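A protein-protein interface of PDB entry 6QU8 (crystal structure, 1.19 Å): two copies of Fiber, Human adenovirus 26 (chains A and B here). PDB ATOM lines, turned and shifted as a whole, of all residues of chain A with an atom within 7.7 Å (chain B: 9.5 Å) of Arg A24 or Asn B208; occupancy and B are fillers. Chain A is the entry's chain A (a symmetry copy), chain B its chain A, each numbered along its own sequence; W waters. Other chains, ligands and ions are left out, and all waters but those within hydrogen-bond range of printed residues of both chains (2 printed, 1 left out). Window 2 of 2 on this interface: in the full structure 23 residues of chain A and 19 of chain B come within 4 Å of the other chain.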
ATOM      1  N   ARG A  24     -12.060 -24.224  22.240  1.00  0.00           N
ATOM      2  CA  ARG A  24     -10.606 -24.540  22.322  1.00  0.00           C
ATOM      3  C   ARG A  24      -9.825 -23.235  22.555  1.00  0.00           C
ATOM      4  O   ARG A  24     -10.403 -22.295  23.147  1.00  0.00           O
ATOM      5  CB  ARG A  24     -10.186 -25.314  21.068  1.00  0.00           C
ATOM      6  CG  ARG A  24     -10.981 -24.956  19.820  1.00  0.00           C
ATOM      7  CD  ARG A  24     -10.548 -23.615  19.266  1.00  0.00           C
ATOM      8  NE  ARG A  24      -9.138 -23.626  18.911  1.00  0.00           N
ATOM      9  CZ  ARG A  24      -8.408 -24.718  18.736  1.00  0.00           C
ATOM     10  NH1 ARG A  24      -8.967 -25.907  18.854  1.00  0.00           N
ATOM     11  NH2 ARG A  24      -7.127 -24.617  18.421  1.00  0.00           N
ATOM     12  N   ARG A  25      -8.557 -23.168  22.132  1.00  0.00           N
ATOM     13  CA  ARG A  25      -7.657 -22.049  22.510  1.00  0.00           C
ATOM     14  C   ARG A  25      -7.133 -21.263  21.307  1.00  0.00           C
ATOM     15  O   ARG A  25      -6.166 -20.548  21.525  1.00  0.00           O
ATOM     16  CB  ARG A  25      -6.446 -22.528  23.313  1.00  0.00           C
ATOM     17  CG  ARG A  25      -5.905 -23.898  22.928  1.00  0.00           C
ATOM     18  CD  ARG A  25      -5.691 -24.724  24.185  1.00  0.00           C
ATOM     19  NE  ARG A  25      -5.253 -23.907  25.309  1.00  0.00           N
ATOM     20  CZ  ARG A  25      -5.946 -22.906  25.849  1.00  0.00           C
ATOM     21  NH1 ARG A  25      -7.130 -22.562  25.366  1.00  0.00           N
ATOM     22  NH2 ARG A  25      -5.437 -22.237  26.868  1.00  0.00           N
ATOM     23  N   THR A  26      -7.802 -21.300  20.152  1.00  0.00           N
ATOM     24  CA  THR A  26      -7.476 -20.443  18.970  1.00  0.00           C
ATOM     25  C   THR A  26      -8.732 -19.800  18.391  1.00  0.00           C
ATOM     26  O   THR A  26      -9.716 -20.506  18.093  1.00  0.00           O
ATOM     27  CB  THR A  26      -6.732 -21.213  17.885  1.00  0.00           C
ATOM     28  OG1 THR A  26      -5.465 -21.562  18.444  1.00  0.00           O
ATOM     29  CG2 THR A  26      -6.490 -20.427  16.624  1.00  0.00           C
ATOM     30  N   LEU A  27      -8.653 -18.490  18.179  1.00  0.00           N
ATOM     31  CA  LEU A  27      -9.614 -17.747  17.337  1.00  0.00           C
ATOM     32  C   LEU A  27      -8.875 -17.409  16.063  1.00  0.00           C
ATOM     33  O   LEU A  27      -7.741 -16.922  16.136  1.00  0.00           O
ATOM     34  CB  LEU A  27     -10.041 -16.418  17.930  1.00  0.00           C
ATOM     35  CG  LEU A  27     -10.943 -16.416  19.132  1.00  0.00           C
ATOM     36  CD1 LEU A  27     -11.180 -14.976  19.568  1.00  0.00           C
ATOM     37  CD2 LEU A  27     -12.269 -17.089  18.814  1.00  0.00           C
ATOM     38  N   TRP A  28      -9.504 -17.597  14.925  1.00  0.00           N
ATOM     39  CA  TRP A  28      -8.794 -17.265  13.690  1.00  0.00           C
ATOM     40  C   TRP A  28      -9.742 -17.001  12.543  1.00  0.00           C
ATOM     41  O   TRP A  28     -10.960 -17.242  12.625  1.00  0.00           O
ATOM     42  CB  TRP A  28      -7.763 -18.344  13.359  1.00  0.00           C
ATOM     43  CG  TRP A  28      -8.285 -19.650  12.846  1.00  0.00           C
ATOM     44  CD1 TRP A  28      -9.569 -20.132  12.815  1.00  0.00           C
ATOM     45  CD2 TRP A  28      -7.459 -20.689  12.307  1.00  0.00           C
ATOM     46  NE1 TRP A  28      -9.591 -21.384  12.259  1.00  0.00           N
ATOM     47  CE2 TRP A  28      -8.309 -21.749  11.935  1.00  0.00           C
ATOM     48  CE3 TRP A  28      -6.085 -20.813  12.087  1.00  0.00           C
ATOM     49  CZ2 TRP A  28      -7.820 -22.918  11.352  1.00  0.00           C
ATOM     50  CZ3 TRP A  28      -5.613 -21.967  11.517  1.00  0.00           C
ATOM     51  CH2 TRP A  28      -6.462 -23.008  11.165  1.00  0.00           C
ATOM     52  N   LEU A  51      -5.210 -15.867  16.753  1.00  0.00           N
ATOM     53  CA  LEU A  51      -5.007 -15.511  18.164  1.00  0.00           C
ATOM     54  C   LEU A  51      -5.021 -16.807  18.978  1.00  0.00           C
ATOM     55  O   LEU A  51      -6.058 -17.479  19.021  1.00  0.00           O
ATOM     56  CB  LEU A  51      -6.113 -14.563  18.609  1.00  0.00           C
ATOM     57  CG  LEU A  51      -6.284 -13.282  17.808  1.00  0.00           C
ATOM     58  CD1 LEU A  51      -7.468 -12.494  18.368  1.00  0.00           C
ATOM     59  CD2 LEU A  51      -5.013 -12.443  17.836  1.00  0.00           C
ATOM     60  N   THR A  52      -3.886 -17.137  19.582  1.00  0.00           N
ATOM     61  CA  THR A  52      -3.757 -18.368  20.377  1.00  0.00           C
ATOM     62  C   THR A  52      -3.595 -17.968  21.839  1.00  0.00           C
ATOM     63  O   THR A  52      -2.719 -17.169  22.190  1.00  0.00           O
ATOM     64  CB  THR A  52      -2.593 -19.205  19.870  1.00  0.00           C
ATOM     65  OG1 THR A  52      -2.825 -19.539  18.504  1.00  0.00           O
ATOM     66  CG2 THR A  52      -2.417 -20.463  20.679  1.00  0.00           C
ATOM     67  N   LYS A  53      -4.463 -18.501  22.664  1.00  0.00           N
ATOM     68  CA  LYS A  53      -4.453 -18.207  24.110  1.00  0.00           C
ATOM     69  C   LYS A  53      -3.330 -18.984  24.776  1.00  0.00           C
ATOM     70  O   LYS A  53      -3.342 -20.198  24.718  1.00  0.00           O
ATOM     71  CB  LYS A  53      -5.819 -18.598  24.663  1.00  0.00           C
ATOM     72  CG  LYS A  53      -5.923 -18.540  26.166  1.00  0.00           C
ATOM     73  CD  LYS A  53      -6.157 -17.169  26.641  1.00  0.00           C
ATOM     74  CE  LYS A  53      -6.716 -17.147  28.041  1.00  0.00           C
ATOM     75  NZ  LYS A  53      -6.549 -15.797  28.609  1.00  0.00           N
ATOM     76  N   ASN A 106     -13.874 -17.162  13.869  1.00  0.00           N
ATOM     77  CA  ASN A 106     -14.422 -17.972  14.972  1.00  0.00           C
ATOM     78  C   ASN A 106     -13.327 -18.869  15.545  1.00  0.00           C
ATOM     79  O   ASN A 106     -12.157 -18.813  15.114  1.00  0.00           O
ATOM     80  CB  ASN A 106     -15.652 -18.763  14.542  1.00  0.00           C
ATOM     81  CG  ASN A 106     -16.750 -18.729  15.590  1.00  0.00           C
ATOM     82  OD1 ASN A 106     -16.501 -18.947  16.781  1.00  0.00           O
ATOM     83  ND2 ASN A 106     -17.964 -18.415  15.169  1.00  0.00           N
ATOM     84  N   TYR A 107     -13.719 -19.642  16.541  1.00  0.00           N
ATOM     85  CA  TYR A 107     -12.842 -20.665  17.132  1.00  0.00           C
ATOM     86  C   TYR A 107     -12.449 -21.647  16.037  1.00  0.00           C
ATOM     87  O   TYR A 107     -13.300 -21.997  15.192  1.00  0.00           O
ATOM     88  CB  TYR A 107     -13.553 -21.347  18.293  1.00  0.00           C
ATOM     89  CG  TYR A 107     -13.593 -20.519  19.548  1.00  0.00           C
ATOM     90  CD1 TYR A 107     -12.515 -20.523  20.404  1.00  0.00           C
ATOM     91  CD2 TYR A 107     -14.689 -19.734  19.883  1.00  0.00           C
ATOM     92  CE1 TYR A 107     -12.523 -19.802  21.581  1.00  0.00           C
ATOM     93  CE2 TYR A 107     -14.700 -18.982  21.049  1.00  0.00           C
ATOM     94  CZ  TYR A 107     -13.623 -19.039  21.912  1.00  0.00           C
ATOM     95  OH  TYR A 107     -13.576 -18.314  23.070  1.00  0.00           O
ATOM     96  N   ARG A 108     -11.208 -22.119  16.077  1.00  0.00           N
ATOM     97  CA  ARG A 108     -10.671 -23.127  15.118  1.00  0.00           C
ATOM     98  C   ARG A 108     -11.328 -24.499  15.333  1.00  0.00           C
ATOM     99  O   ARG A 108     -11.621 -24.855  16.493  1.00  0.00           O
ATOM    100  CB  ARG A 108      -9.149 -23.259  15.262  1.00  0.00           C
ATOM    101  CG  ARG A 108      -8.547 -24.362  14.394  1.00  0.00           C
ATOM    102  CD  ARG A 108      -7.026 -24.452  14.431  1.00  0.00           C
ATOM    103  NE  ARG A 108      -6.492 -25.161  13.264  1.00  0.00           N
ATOM    104  CZ  ARG A 108      -5.245 -25.618  13.127  1.00  0.00           C
ATOM    105  NH1 ARG A 108      -4.364 -25.485  14.103  1.00  0.00           N
ATOM    106  NH2 ARG A 108      -4.880 -26.237  12.014  1.00  0.00           N
ATOM    107  N   SER A 109     -11.533 -25.231  14.230  1.00  0.00           N
ATOM    108  CA  SER A 109     -11.709 -26.708  14.162  1.00  0.00           C
ATOM    109  C   SER A 109     -11.086 -27.199  12.847  1.00  0.00           C
ATOM    110  O   SER A 109     -11.483 -26.668  11.786  1.00  0.00           O
ATOM    111  CB  SER A 109     -13.159 -27.095  14.277  1.00  0.00           C
ATOM    112  OG  SER A 109     -13.967 -26.198  13.533  1.00  0.00           O
ATOM    113  N   ASP A 110     -10.131 -28.137  12.923  1.00  0.00           N
ATOM    114  CA  ASP A 110      -9.278 -28.592  11.787  1.00  0.00           C
ATOM    115  C   ASP A 110      -8.633 -27.351  11.143  1.00  0.00           C
ATOM    116  O   ASP A 110      -8.005 -26.592  11.896  1.00  0.00           O
ATOM    117  CB  ASP A 110     -10.084 -29.486  10.840  1.00  0.00           C
ATOM    118  CG  ASP A 110     -10.509 -30.805  11.466  1.00  0.00           C
ATOM    119  OD1 ASP A 110     -10.517 -30.891  12.715  1.00  0.00           O
ATOM    120  OD2 ASP A 110     -10.820 -31.740  10.702  1.00  0.00           O
ATOM    121  N   SER A 112     -10.594 -25.136   9.596  1.00  0.00           N
ATOM    122  CA  SER A 112     -11.834 -24.330   9.419  1.00  0.00           C
ATOM    123  C   SER A 112     -12.235 -23.651  10.736  1.00  0.00           C
ATOM    124  O   SER A 112     -11.363 -23.447  11.596  1.00  0.00           O
ATOM    125  CB  SER A 112     -12.942 -25.185   8.857  1.00  0.00           C
ATOM    126  OG  SER A 112     -14.046 -24.389   8.437  1.00  0.00           O
ATOM    127  N   VAL A 114     -15.601 -23.346  13.878  1.00  0.00           N
ATOM    128  CA  VAL A 114     -16.768 -24.067  14.479  1.00  0.00           C
ATOM    129  C   VAL A 114     -18.059 -23.575  13.804  1.00  0.00           C
ATOM    130  O   VAL A 114     -18.029 -22.502  13.159  1.00  0.00           O
ATOM    131  CB  VAL A 114     -16.824 -23.905  16.015  1.00  0.00           C
ATOM    132  CG1 VAL A 114     -15.597 -24.500  16.689  1.00  0.00           C
ATOM    133  CG2 VAL A 114     -17.010 -22.458  16.446  1.00  0.00           C
ATOM    134  N   ASN A 120     -18.626 -16.914  23.413  1.00  0.00           N
ATOM    135  CA  ASN A 120     -17.884 -15.994  24.326  1.00  0.00           C
ATOM    136  C   ASN A 120     -16.392 -16.122  24.048  1.00  0.00           C
ATOM    137  O   ASN A 120     -15.900 -17.252  23.893  1.00  0.00           O
ATOM    138  CB  ASN A 120     -18.117 -16.327  25.807  1.00  0.00           C
ATOM    139  CG  ASN A 120     -17.398 -15.447  26.825  1.00  0.00           C
ATOM    140  OD1 ASN A 120     -16.161 -15.477  27.012  1.00  0.00           O
ATOM    141  ND2 ASN A 120     -18.200 -14.716  27.576  1.00  0.00           N
ATOM    142  N   PHE A 124      -9.780 -13.934  25.250  1.00  0.00           N
ATOM    143  CA  PHE A 124      -8.943 -13.476  24.116  1.00  0.00           C
ATOM    144  C   PHE A 124      -8.903 -11.957  24.046  1.00  0.00           C
ATOM    145  O   PHE A 124      -8.188 -11.437  23.171  1.00  0.00           O
ATOM    146  CB  PHE A 124      -9.447 -14.007  22.784  1.00  0.00           C
ATOM    147  CG  PHE A 124      -9.269 -15.490  22.643  1.00  0.00           C
ATOM    148  CD1 PHE A 124     -10.192 -16.361  23.202  1.00  0.00           C
ATOM    149  CD2 PHE A 124      -8.206 -16.020  21.932  1.00  0.00           C
ATOM    150  CE1 PHE A 124     -10.028 -17.727  23.098  1.00  0.00           C
ATOM    151  CE2 PHE A 124      -8.064 -17.389  21.801  1.00  0.00           C
ATOM    152  CZ  PHE A 124      -8.981 -18.236  22.373  1.00  0.00           C
ATOM    153  N   ARG B  25       6.534 -31.087  24.037  1.00  0.00           N
ATOM    154  CA  ARG B  25       6.065 -29.951  23.205  1.00  0.00           C
ATOM    155  C   ARG B  25       7.193 -29.013  22.771  1.00  0.00           C
ATOM    156  O   ARG B  25       6.840 -27.918  22.361  1.00  0.00           O
ATOM    157  CB  ARG B  25       5.011 -29.105  23.923  1.00  0.00           C
ATOM    158  CG  ARG B  25       5.190 -28.976  25.429  1.00  0.00           C
ATOM    159  CD  ARG B  25       3.862 -29.247  26.116  1.00  0.00           C
ATOM    160  NE  ARG B  25       2.732 -28.760  25.336  1.00  0.00           N
ATOM    161  CZ  ARG B  25       2.406 -29.175  24.113  1.00  0.00           C
ATOM    162  NH1 ARG B  25       3.132 -30.090  23.491  1.00  0.00           N
ATOM    163  NH2 ARG B  25       1.355 -28.652  23.506  1.00  0.00           N
ATOM    164  N   LYS B  53       5.532 -25.859  20.798  1.00  0.00           N
ATOM    165  CA  LYS B  53       4.135 -25.992  20.342  1.00  0.00           C
ATOM    166  C   LYS B  53       3.212 -25.302  21.333  1.00  0.00           C
ATOM    167  O   LYS B  53       3.189 -25.692  22.484  1.00  0.00           O
ATOM    168  CB  LYS B  53       3.834 -27.482  20.230  1.00  0.00           C
ATOM    169  CG  LYS B  53       2.388 -27.807  19.955  1.00  0.00           C
ATOM    170  CD  LYS B  53       2.061 -27.663  18.529  1.00  0.00           C
ATOM    171  CE  LYS B  53       0.801 -28.407  18.163  1.00  0.00           C
ATOM    172  NZ  LYS B  53       0.304 -27.912  16.866  1.00  0.00           N
ATOM    173  N   CYS B  54       2.466 -24.315  20.849  1.00  0.00           N
ATOM    174  CA  CYS B  54       1.417 -23.567  21.577  1.00  0.00           C
ATOM    175  C   CYS B  54       0.103 -23.731  20.788  1.00  0.00           C
ATOM    176  O   CYS B  54      -0.262 -22.815  20.035  1.00  0.00           O
ATOM    177  CB  CYS B  54       1.810 -22.102  21.743  1.00  0.00           C
ATOM    178  SG  CYS B  54       3.503 -21.836  22.350  1.00  0.00           S
ATOM    179  N   GLY B  55      -0.520 -24.909  20.837  1.00  0.00           N
ATOM    180  CA  GLY B  55      -1.763 -25.158  20.093  1.00  0.00           C
ATOM    181  C   GLY B  55      -1.572 -25.003  18.597  1.00  0.00           C
ATOM    182  O   GLY B  55      -0.725 -25.669  18.018  1.00  0.00           O
ATOM    183  N   SER B  56      -2.341 -24.086  18.022  1.00  0.00           N
ATOM    184  CA  SER B  56      -2.417 -23.780  16.575  1.00  0.00           C
ATOM    185  C   SER B  56      -1.079 -23.220  16.077  1.00  0.00           C
ATOM    186  O   SER B  56      -0.839 -23.313  14.866  1.00  0.00           O
ATOM    187  CB  SER B  56      -3.574 -22.833  16.333  1.00  0.00           C
ATOM    188  OG  SER B  56      -3.579 -21.788  17.303  1.00  0.00           O
ATOM    189  N   GLN B  57      -0.249 -22.660  16.971  1.00  0.00           N
ATOM    190  CA  GLN B  57       0.996 -21.980  16.572  1.00  0.00           C
ATOM    191  C   GLN B  57       2.205 -22.652  17.219  1.00  0.00           C
ATOM    192  O   GLN B  57       2.108 -23.250  18.288  1.00  0.00           O
ATOM    193  CB  GLN B  57       1.009 -20.491  16.912  1.00  0.00           C
ATOM    194  CG  GLN B  57       0.029 -19.670  16.099  1.00  0.00           C
ATOM    195  CD  GLN B  57       0.062 -18.212  16.498  1.00  0.00           C
ATOM    196  OE1 GLN B  57       1.039 -17.500  16.259  1.00  0.00           O
ATOM    197  NE2 GLN B  57      -0.984 -17.768  17.165  1.00  0.00           N
ATOM    198  N   VAL B  58       3.334 -22.534  16.555  1.00  0.00           N
ATOM    199  CA  VAL B  58       4.659 -22.757  17.152  1.00  0.00           C
ATOM    200  C   VAL B  58       5.236 -21.388  17.509  1.00  0.00           C
ATOM    201  O   VAL B  58       5.180 -20.471  16.680  1.00  0.00           O
ATOM    202  CB  VAL B  58       5.567 -23.540  16.197  1.00  0.00           C
ATOM    203  CG1 VAL B  58       7.049 -23.319  16.490  1.00  0.00           C
ATOM    204  CG2 VAL B  58       5.231 -25.006  16.282  1.00  0.00           C
ATOM    205  N   ALA B 121       6.612 -35.444  13.921  1.00  0.00           N
ATOM    206  CA  ALA B 121       6.583 -34.039  14.361  1.00  0.00           C
ATOM    207  C   ALA B 121       5.643 -33.225  13.468  1.00  0.00           C
ATOM    208  O   ALA B 121       5.847 -32.011  13.355  1.00  0.00           O
ATOM    209  CB  ALA B 121       7.982 -33.479  14.374  1.00  0.00           C
ATOM    210  N   VAL B 122       4.616 -33.851  12.898  1.00  0.00           N
ATOM    211  CA  VAL B 122       3.659 -33.117  12.034  1.00  0.00           C
ATOM    212  C   VAL B 122       3.054 -31.926  12.779  1.00  0.00           C
ATOM    213  O   VAL B 122       2.902 -30.874  12.179  1.00  0.00           O
ATOM    214  CB  VAL B 122       2.611 -34.048  11.416  1.00  0.00           C
ATOM    215  CG1 VAL B 122       1.567 -33.269  10.638  1.00  0.00           C
ATOM    216  CG2 VAL B 122       3.261 -35.096  10.530  1.00  0.00           C
ATOM    217  N   PRO B 123       2.721 -31.997  14.085  1.00  0.00           N
ATOM    218  CA  PRO B 123       2.141 -30.842  14.772  1.00  0.00           C
ATOM    219  C   PRO B 123       3.069 -29.626  14.875  1.00  0.00           C
ATOM    220  O   PRO B 123       2.598 -28.580  15.291  1.00  0.00           O
ATOM    221  CB  PRO B 123       1.770 -31.413  16.154  1.00  0.00           C
ATOM    222  CG  PRO B 123       1.554 -32.882  15.875  1.00  0.00           C
ATOM    223  CD  PRO B 123       2.690 -33.211  14.931  1.00  0.00           C
ATOM    224  N   PHE B 124       4.346 -29.781  14.552  1.00  0.00           N
ATOM    225  CA  PHE B 124       5.324 -28.668  14.514  1.00  0.00           C
ATOM    226  C   PHE B 124       5.488 -28.132  13.099  1.00  0.00           C
ATOM    227  O   PHE B 124       6.240 -27.156  12.934  1.00  0.00           O
ATOM    228  CB  PHE B 124       6.690 -29.090  15.031  1.00  0.00           C
ATOM    229  CG  PHE B 124       6.693 -29.376  16.503  1.00  0.00           C
ATOM    230  CD1 PHE B 124       6.266 -30.608  16.977  1.00  0.00           C
ATOM    231  CD2 PHE B 124       7.146 -28.438  17.415  1.00  0.00           C
ATOM    232  CE1 PHE B 124       6.244 -30.875  18.330  1.00  0.00           C
ATOM    233  CE2 PHE B 124       7.154 -28.722  18.767  1.00  0.00           C
ATOM    234  CZ  PHE B 124       6.715 -29.943  19.219  1.00  0.00           C
ATOM    235  N   MET B 125       4.899 -28.773  12.104  1.00  0.00           N
ATOM    236  CA  MET B 125       5.168 -28.376  10.715  1.00  0.00           C
ATOM    237  C   MET B 125       4.336 -27.167  10.332  1.00  0.00           C
ATOM    238  O   MET B 125       3.202 -26.979  10.789  1.00  0.00           O
ATOM    239  CB  MET B 125       4.900 -29.535   9.767  1.00  0.00           C
ATOM    240  CG  MET B 125       5.904 -30.671   9.965  1.00  0.00           C
ATOM    241  SD  MET B 125       7.599 -30.218   9.565  1.00  0.00           S
ATOM    242  CE  MET B 125       8.330 -30.045  11.185  1.00  0.00           C
ATOM    243  N   ASN B 127       1.769 -24.941   8.466  1.00  0.00           N
ATOM    244  CA  ASN B 127       0.457 -25.248   7.854  1.00  0.00           C
ATOM    245  C   ASN B 127       0.516 -25.083   6.335  1.00  0.00           C
ATOM    246  O   ASN B 127       0.899 -24.004   5.870  1.00  0.00           O
ATOM    247  CB  ASN B 127      -0.573 -24.317   8.497  1.00  0.00           C
ATOM    248  CG  ASN B 127      -1.983 -24.648   8.075  1.00  0.00           C
ATOM    249  OD1 ASN B 127      -2.403 -24.298   6.972  1.00  0.00           O
ATOM    250  ND2 ASN B 127      -2.719 -25.275   8.982  1.00  0.00           N
ATOM    251  N   LEU B 204       1.725 -20.743  11.978  1.00  0.00           N
ATOM    252  CA  LEU B 204       0.555 -21.636  12.037  1.00  0.00           C
ATOM    253  C   LEU B 204       1.007 -23.063  11.745  1.00  0.00           C
ATOM    254  O   LEU B 204       1.761 -23.267  10.772  1.00  0.00           O
ATOM    255  CB  LEU B 204      -0.477 -21.183  11.001  1.00  0.00           C
ATOM    256  CG  LEU B 204      -1.379 -20.014  11.417  1.00  0.00           C
ATOM    257  CD1 LEU B 204      -0.635 -18.809  11.959  1.00  0.00           C
ATOM    258  CD2 LEU B 204      -2.260 -19.588  10.251  1.00  0.00           C
ATOM    259  N   THR B 205       0.509 -24.028  12.520  1.00  0.00           N
ATOM    260  CA  THR B 205       0.922 -25.431  12.346  1.00  0.00           C
ATOM    261  C   THR B 205      -0.098 -26.222  11.539  1.00  0.00           C
ATOM    262  O   THR B 205      -1.305 -25.894  11.476  1.00  0.00           O
ATOM    263  CB  THR B 205       1.163 -26.098  13.695  1.00  0.00           C
ATOM    264  OG1 THR B 205      -0.080 -26.126  14.401  1.00  0.00           O
ATOM    265  CG2 THR B 205       2.179 -25.358  14.521  1.00  0.00           C
ATOM    266  N   GLN B 206       0.422 -27.299  10.971  1.00  0.00           N
ATOM    267  CA  GLN B 206      -0.363 -28.295  10.230  1.00  0.00           C
ATOM    268  C   GLN B 206      -1.374 -28.942  11.153  1.00  0.00           C
ATOM    269  O   GLN B 206      -2.511 -29.236  10.659  1.00  0.00           O
ATOM    270  CB  GLN B 206       0.609 -29.272   9.550  1.00  0.00           C
ATOM    271  CG  GLN B 206      -0.022 -30.293   8.633  1.00  0.00           C
ATOM    272  CD  GLN B 206      -0.580 -29.767   7.345  1.00  0.00           C
ATOM    273  OE1 GLN B 206      -1.174 -30.518   6.593  1.00  0.00           O
ATOM    274  NE2 GLN B 206      -0.558 -28.480   7.136  1.00  0.00           N
ATOM    275  N   GLU B 207      -1.039 -29.215  12.406  1.00  0.00           N
ATOM    276  CA  GLU B 207      -2.023 -29.964  13.253  1.00  0.00           C
ATOM    277  C   GLU B 207      -2.049 -29.396  14.677  1.00  0.00           C
ATOM    278  O   GLU B 207      -1.236 -28.506  14.970  1.00  0.00           O
ATOM    279  CB  GLU B 207      -1.721 -31.465  13.205  1.00  0.00           C
ATOM    280  CG  GLU B 207      -2.350 -32.182  12.015  1.00  0.00           C
ATOM    281  CD  GLU B 207      -1.872 -33.610  11.812  1.00  0.00           C
ATOM    282  OE1 GLU B 207      -2.142 -34.173  10.729  1.00  0.00           O
ATOM    283  OE2 GLU B 207      -1.222 -34.159  12.734  1.00  0.00           O
ATOM    284  N   ASN B 208      -2.983 -29.877  15.504  1.00  0.00           N
ATOM    285  CA  ASN B 208      -3.240 -29.396  16.891  1.00  0.00           C
ATOM    286  C   ASN B 208      -4.249 -30.336  17.564  1.00  0.00           C
ATOM    287  O   ASN B 208      -3.884 -31.404  18.053  1.00  0.00           O
ATOM    288  CB  ASN B 208      -3.727 -27.942  16.898  1.00  0.00           C
ATOM    289  CG  ASN B 208      -4.130 -27.438  18.269  1.00  0.00           C
ATOM    290  OD1 ASN B 208      -4.874 -26.462  18.378  1.00  0.00           O
ATOM    291  ND2 ASN B 208      -3.651 -28.088  19.321  1.00  0.00           N
HETATM  292  O   HOH W   1      -4.855 -23.648  19.672  1.00  0.00           O
HETATM  293  O   HOH W   2      -6.976 -27.064  16.717  1.00  0.00           O
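The side-chain hydroxyl of Thr A52 is in hydrogen-bond range of the side-chain amide nitrogen of Gln B57 (2.9 Å).
The side-chain hydroxyl (OG) of Ser B56 sits close to the side-chain hydroxyl (OG1) of Thr A26 (2.2 Å).
OG of Ser B56 is in hydrogen-bond range of OG1 of Thr A52 (2.7 Å).
The side-chain amide oxygen of Asn B208 lies within hydrogen-bond range of the guanidinium group of Arg A24 (2.9 Å).
The backbone carbonyl oxygen (O) of Thr A26 sits at hydrogen-bond distance from the guanidinium group (NE) of Arg A24, 3.3 Å away.
The side-chain hydroxyl of Thr B205 is in hydrogen-bond range of the side-chain amino group of Lys B53, 3.1 Å away.
N of Ser B56 sits at hydrogen-bond distance from OD1 of Asn B208, at 3.5 Å.
The backbone carbonyl oxygen (O) of Ser B56 sits at hydrogen-bond distance from the backbone NH (N) of Thr B205 (2.8 Å).
The guanidinium group (NE) of Arg A108 lies within hydrogen-bond range of the backbone carbonyl oxygen (O) of Asp A110 (2.5 Å).
The side-chain hydroxyl of Thr B205 lies within hydrogen-bond range of the backbone carbonyl oxygen of Glu B207, 2.7 Å away.
O of Cys B54 touches CG2 of Thr A52, 3.3 Å away.
Arg A108 touches Ser B56.
ND2 of Asn B127 touches NH2 of Arg A108 (3.8 Å).
O of Thr B205 touches NH2 of Arg A108, at 3.6 Å.
Asn B208 touches Arg A108 (CB to NH1, 3.8 Å).
Of the printed residues of chain B, Arg A24 touches Asn B208 (2.9 Å).
Of the printed residues of chain A, Cys B54 touches Thr A52 (3.3 Å).
Printed residues of chain A within 4 Å of Asn B127: Arg A108 (3.8 Å).
Printed residues of chain A within 4 Å of Gln B57: Thr A52.
The nearest printed residue of chain A that does not touch Asn B208 is Thr A26 (4.9 Å).
Among the printed residues, 9 pairs touch across the chains.
Among the printed residues, no Asp or Glu carboxylate lies within 4 Å of a Lys or Arg side-chain nitrogen of the other chain.
3 positions are printed for both chains.
Of the 9 pairs that touch across the chains among the printed residues, none has its exchanged pair printed and touching as well.
Water W1 lies within hydrogen-bond range of OG1 of Thr A26 (2.5 Å), NH2 of Arg A24 (2.8 Å), N of Ser B56 (3.0 Å) and OD1 of Asn B208 (3.1 Å).
Water W2 bridges the side-chain amide oxygen of Asn B208 (2.7 Å) and the guanidinium group of Arg A24 (3.0 Å).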
